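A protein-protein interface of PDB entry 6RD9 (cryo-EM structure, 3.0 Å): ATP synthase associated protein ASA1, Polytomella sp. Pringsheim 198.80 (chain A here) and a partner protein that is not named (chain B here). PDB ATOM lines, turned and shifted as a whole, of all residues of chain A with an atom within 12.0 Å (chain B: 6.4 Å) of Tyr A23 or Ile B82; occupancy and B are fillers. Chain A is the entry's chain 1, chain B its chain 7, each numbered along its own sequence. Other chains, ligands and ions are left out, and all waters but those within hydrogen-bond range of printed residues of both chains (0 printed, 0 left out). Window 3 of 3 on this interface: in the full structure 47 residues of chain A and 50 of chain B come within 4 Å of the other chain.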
ATOM      1  N   TYR A  23      -3.243  16.855  14.650  1.00  0.00           N
ATOM      2  CA  TYR A  23      -4.483  16.357  15.210  1.00  0.00           C
ATOM      3  C   TYR A  23      -5.113  17.401  16.087  1.00  0.00           C
ATOM      4  O   TYR A  23      -6.259  17.280  16.482  1.00  0.00           O
ATOM      5  CB  TYR A  23      -4.249  15.082  16.008  1.00  0.00           C
ATOM      6  CG  TYR A  23      -3.135  15.153  17.017  1.00  0.00           C
ATOM      7  CD1 TYR A  23      -1.876  14.692  16.703  1.00  0.00           C
ATOM      8  CD2 TYR A  23      -3.349  15.656  18.287  1.00  0.00           C
ATOM      9  CE1 TYR A  23      -0.866  14.743  17.608  1.00  0.00           C
ATOM     10  CE2 TYR A  23      -2.342  15.713  19.195  1.00  0.00           C
ATOM     11  CZ  TYR A  23      -1.104  15.255  18.849  1.00  0.00           C
ATOM     12  OH  TYR A  23      -0.082  15.301  19.754  1.00  0.00           O
ATOM     13  N   LEU A  24      -4.345  18.417  16.423  1.00  0.00           N
ATOM     14  CA  LEU A  24      -4.793  19.436  17.353  1.00  0.00           C
ATOM     15  C   LEU A  24      -5.365  20.647  16.634  1.00  0.00           C
ATOM     16  O   LEU A  24      -5.000  20.958  15.501  1.00  0.00           O
ATOM     17  CB  LEU A  24      -3.657  19.824  18.297  1.00  0.00           C
ATOM     18  CG  LEU A  24      -2.226  19.795  17.795  1.00  0.00           C
ATOM     19  CD1 LEU A  24      -1.940  20.926  16.930  1.00  0.00           C
ATOM     20  CD2 LEU A  24      -1.341  19.867  18.991  1.00  0.00           C
ATOM     21  N   ALA A  25      -6.275  21.319  17.312  1.00  0.00           N
ATOM     22  CA  ALA A  25      -7.126  22.342  16.748  1.00  0.00           C
ATOM     23  C   ALA A  25      -6.774  23.710  17.305  1.00  0.00           C
ATOM     24  O   ALA A  25      -6.169  23.818  18.376  1.00  0.00           O
ATOM     25  CB  ALA A  25      -8.591  22.014  17.059  1.00  0.00           C
ATOM     26  N   PRO A  26      -7.113  24.786  16.598  1.00  0.00           N
ATOM     27  CA  PRO A  26      -7.021  26.113  17.207  1.00  0.00           C
ATOM     28  C   PRO A  26      -8.091  26.292  18.269  1.00  0.00           C
ATOM     29  O   PRO A  26      -9.260  25.973  18.053  1.00  0.00           O
ATOM     30  CB  PRO A  26      -7.237  27.062  16.027  1.00  0.00           C
ATOM     31  CG  PRO A  26      -7.922  26.255  15.021  1.00  0.00           C
ATOM     32  CD  PRO A  26      -7.396  24.877  15.161  1.00  0.00           C
ATOM     33  N   LEU A  27      -7.683  26.795  19.424  1.00  0.00           N
ATOM     34  CA  LEU A  27      -8.622  27.044  20.501  1.00  0.00           C
ATOM     35  C   LEU A  27      -9.355  28.353  20.256  1.00  0.00           C
ATOM     36  O   LEU A  27      -8.736  29.368  19.933  1.00  0.00           O
ATOM     37  CB  LEU A  27      -7.894  27.086  21.838  1.00  0.00           C
ATOM     38  CG  LEU A  27      -7.338  25.790  22.404  1.00  0.00           C
ATOM     39  CD1 LEU A  27      -6.944  25.990  23.837  1.00  0.00           C
ATOM     40  CD2 LEU A  27      -8.343  24.683  22.290  1.00  0.00           C
ATOM     41  N   ALA B  80     -10.819   8.064  25.172  1.00  0.00           N
ATOM     42  CA  ALA B  80     -10.611   8.472  23.801  1.00  0.00           C
ATOM     43  C   ALA B  80      -9.207   9.010  23.640  1.00  0.00           C
ATOM     44  O   ALA B  80      -8.562   9.402  24.610  1.00  0.00           O
ATOM     45  CB  ALA B  80     -11.630   9.522  23.395  1.00  0.00           C
ATOM     46  N   ARG B  81      -8.721   8.992  22.405  1.00  0.00           N
ATOM     47  CA  ARG B  81      -7.383   9.500  22.155  1.00  0.00           C
ATOM     48  C   ARG B  81      -7.346  10.998  22.334  1.00  0.00           C
ATOM     49  O   ARG B  81      -6.472  11.528  23.018  1.00  0.00           O
ATOM     50  CB  ARG B  81      -6.918   9.132  20.759  1.00  0.00           C
ATOM     51  CG  ARG B  81      -5.617   9.761  20.417  1.00  0.00           C
ATOM     52  CD  ARG B  81      -4.993   9.110  19.255  1.00  0.00           C
ATOM     53  NE  ARG B  81      -3.769   9.784  18.867  1.00  0.00           N
ATOM     54  CZ  ARG B  81      -3.703  10.664  17.885  1.00  0.00           C
ATOM     55  NH1 ARG B  81      -2.558  11.233  17.577  1.00  0.00           N
ATOM     56  NH2 ARG B  81      -4.794  10.972  17.214  1.00  0.00           N
ATOM     57  N   ILE B  82      -8.307  11.693  21.751  1.00  0.00           N
ATOM     58  CA  ILE B  82      -8.451  13.127  21.914  1.00  0.00           C
ATOM     59  C   ILE B  82      -9.738  13.464  22.645  1.00  0.00           C
ATOM     60  O   ILE B  82      -9.705  13.969  23.762  1.00  0.00           O
ATOM     61  CB  ILE B  82      -8.355  13.847  20.557  1.00  0.00           C
ATOM     62  CG1 ILE B  82      -6.953  13.659  20.016  1.00  0.00           C
ATOM     63  CG2 ILE B  82      -8.645  15.290  20.720  1.00  0.00           C
ATOM     64  CD1 ILE B  82      -6.735  14.250  18.701  1.00  0.00           C
ATOM     65  N   SER B  83     -10.879  13.130  22.064  1.00  0.00           N
ATOM     66  CA  SER B  83     -12.150  13.309  22.742  1.00  0.00           C
ATOM     67  C   SER B  83     -13.149  12.378  22.090  1.00  0.00           C
ATOM     68  O   SER B  83     -12.849  11.731  21.095  1.00  0.00           O
ATOM     69  CB  SER B  83     -12.619  14.758  22.693  1.00  0.00           C
ATOM     70  OG  SER B  83     -12.671  15.246  21.378  1.00  0.00           O
ATOM     71  N   VAL B  84     -14.323  12.275  22.694  1.00  0.00           N
ATOM     72  CA  VAL B  84     -15.378  11.460  22.119  1.00  0.00           C
ATOM     73  C   VAL B  84     -15.979  12.143  20.911  1.00  0.00           C
ATOM     74  O   VAL B  84     -16.430  11.478  19.979  1.00  0.00           O
ATOM     75  CB  VAL B  84     -16.427  11.163  23.191  1.00  0.00           C
ATOM     76  CG1 VAL B  84     -17.391  10.170  22.720  1.00  0.00           C
ATOM     77  CG2 VAL B  84     -15.753  10.611  24.374  1.00  0.00           C
ATOM     78  N   HIS B  86     -14.269  14.154  18.746  1.00  0.00           N
ATOM     79  CA  HIS B  86     -13.287  14.032  17.687  1.00  0.00           C
ATOM     80  C   HIS B  86     -13.229  12.627  17.138  1.00  0.00           C
ATOM     81  O   HIS B  86     -13.096  12.443  15.934  1.00  0.00           O
ATOM     82  CB  HIS B  86     -11.945  14.441  18.246  1.00  0.00           C
ATOM     83  CG  HIS B  86     -10.825  14.359  17.275  1.00  0.00           C
ATOM     84  ND1 HIS B  86     -10.322  15.465  16.642  1.00  0.00           N
ATOM     85  CD2 HIS B  86     -10.070  13.316  16.870  1.00  0.00           C
ATOM     86  CE1 HIS B  86      -9.326  15.101  15.864  1.00  0.00           C
ATOM     87  NE2 HIS B  86      -9.151  13.803  15.987  1.00  0.00           N
ATOM     88  N   SER B  87     -13.354  11.631  17.995  1.00  0.00           N
ATOM     89  CA  SER B  87     -13.321  10.248  17.566  1.00  0.00           C
ATOM     90  C   SER B  87     -14.549   9.852  16.791  1.00  0.00           C
ATOM     91  O   SER B  87     -14.520   8.850  16.095  1.00  0.00           O
ATOM     92  CB  SER B  87     -13.179   9.353  18.773  1.00  0.00           C
ATOM     93  OG  SER B  87     -11.908   9.543  19.343  1.00  0.00           O
ATOM     94  N   SER B 151      -7.080  11.900  11.230  1.00  0.00           N
ATOM     95  CA  SER B 151      -7.204  12.442  12.568  1.00  0.00           C
ATOM     96  C   SER B 151      -6.933  13.921  12.626  1.00  0.00           C
ATOM     97  O   SER B 151      -7.289  14.548  13.614  1.00  0.00           O
ATOM     98  CB  SER B 151      -6.257  11.745  13.521  1.00  0.00           C
ATOM     99  OG  SER B 151      -6.149  12.489  14.710  1.00  0.00           O
ATOM    100  N   ALA B 152      -6.297  14.491  11.621  1.00  0.00           N
ATOM    101  CA  ALA B 152      -6.112  15.925  11.563  1.00  0.00           C
ATOM    102  C   ALA B 152      -7.129  16.598  10.679  1.00  0.00           C
ATOM    103  O   ALA B 152      -7.227  17.822  10.707  1.00  0.00           O
ATOM    104  CB  ALA B 152      -4.716  16.265  11.062  1.00  0.00           C
ATOM    105  N   LEU B 153      -7.856  15.833   9.876  1.00  0.00           N
ATOM    106  CA  LEU B 153      -9.010  16.378   9.184  1.00  0.00           C
ATOM    107  C   LEU B 153     -10.200  16.479  10.102  1.00  0.00           C
ATOM    108  O   LEU B 153     -11.120  17.249   9.833  1.00  0.00           O
ATOM    109  CB  LEU B 153      -9.403  15.509   8.008  1.00  0.00           C
ATOM    110  CG  LEU B 153      -8.543  15.318   6.796  1.00  0.00           C
ATOM    111  CD1 LEU B 153      -9.346  14.481   5.898  1.00  0.00           C
ATOM    112  CD2 LEU B 153      -8.302  16.642   6.198  1.00  0.00           C
ATOM    113  N   ALA B 154     -10.234  15.673  11.152  1.00  0.00           N
ATOM    114  CA  ALA B 154     -11.308  15.776  12.112  1.00  0.00           C
ATOM    115  C   ALA B 154     -11.168  17.010  12.973  1.00  0.00           C
ATOM    116  O   ALA B 154     -12.165  17.491  13.497  1.00  0.00           O
ATOM    117  CB  ALA B 154     -11.344  14.532  12.973  1.00  0.00           C
ATOM    118  N   SER B 155      -9.967  17.540  13.123  1.00  0.00           N
ATOM    119  CA  SER B 155      -9.744  18.774  13.854  1.00  0.00           C
ATOM    120  C   SER B 155     -10.012  20.013  13.034  1.00  0.00           C
ATOM    121  O   SER B 155      -9.829  21.118  13.536  1.00  0.00           O
ATOM    122  CB  SER B 155      -8.322  18.829  14.353  1.00  0.00           C
ATOM    123  OG  SER B 155      -8.116  17.828  15.304  1.00  0.00           O
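Tyr A23 touches just these residues of chain B: Arg B81 (3.6 Å), Ile B82 (3.7 Å), His B86 (3.8 Å), Ser B151 (3.5 Å), Ala B152 (3.9 Å) and Ser B155 (2.3 Å). Printed residues of chain A within 4 Å of Ile B82: Tyr A23 (3.7 Å). Arg B81 touches just one residue of chain A: Tyr A23 (3.6 Å). His B86 touches one residue of chain A. Of chain A, only Tyr A23 (3.5 Å) comes within 4 Å of Ser B151. No residue of chain A comes within 4 Å of Ala B154. Of chain A, only Tyr A23 (2.3 Å), Leu A24 (3.98 Å) and Ala A25 (3.8 Å) come within 4 Å of Ser B155. Printed residues of chain B within 4 Å of Ala A25: Ser B155. Printed residues of chain B within 4 Å of Leu A24: Ser B155. Pro A26 touches none of the printed residues of chain B. Ser B87 touches none of the printed residues of chain A. The nearest residue of chain B that does not touch Tyr A23 is Ala B154 (6.0 Å). The nearest residue of chain A that does not touch Ile B82 is Leu A24 (5.3 Å).
Of the 12 printed residues of chain B, 6 touch a printed residue of chain A. Hydrophobic or aromatic side chains of chain B within 4 Å of the printed part of chain A: Ile B82, His B86 and Ala B152. Hydrophobic or aromatic side chains of chain A within 4 Å of the printed part of chain B: Tyr A23 and Ala A25. Among the printed residues, 8 pairs touch across the chains.
O of Tyr A23 lies close to OG of Ser B155 (2.3 Å).
A ring nitrogen (ND1) of His B86 sits close to the side-chain hydroxyl of Ser B155. The backbone NH of His B86 lies within hydrogen-bond range of the side-chain hydroxyl of Ser B83 (3.3 Å). The side-chain hydroxyl (OG) of Ser B151 sits at hydrogen-bond distance from the guanidinium group (NH2) of Arg B81 (3.2 Å). O of Ser B151 lies close to NE2 of His B86 (3.1 Å).
Tyr A23 touches Arg B81 (CD1 to NH1, 3.6 Å). Tyr A23 touches Ile B82. Tyr A23 touches His B86 (O to CE1, 3.8 Å). Tyr A23 touches Ser B151. N of Tyr A23 touches CB of Ala B152, at 3.9 Å. OG of Ser B155 touches N of Leu A24, at 3.98 Å. CB of Ala A25 touches O of Ser B155, at 3.8 Å.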
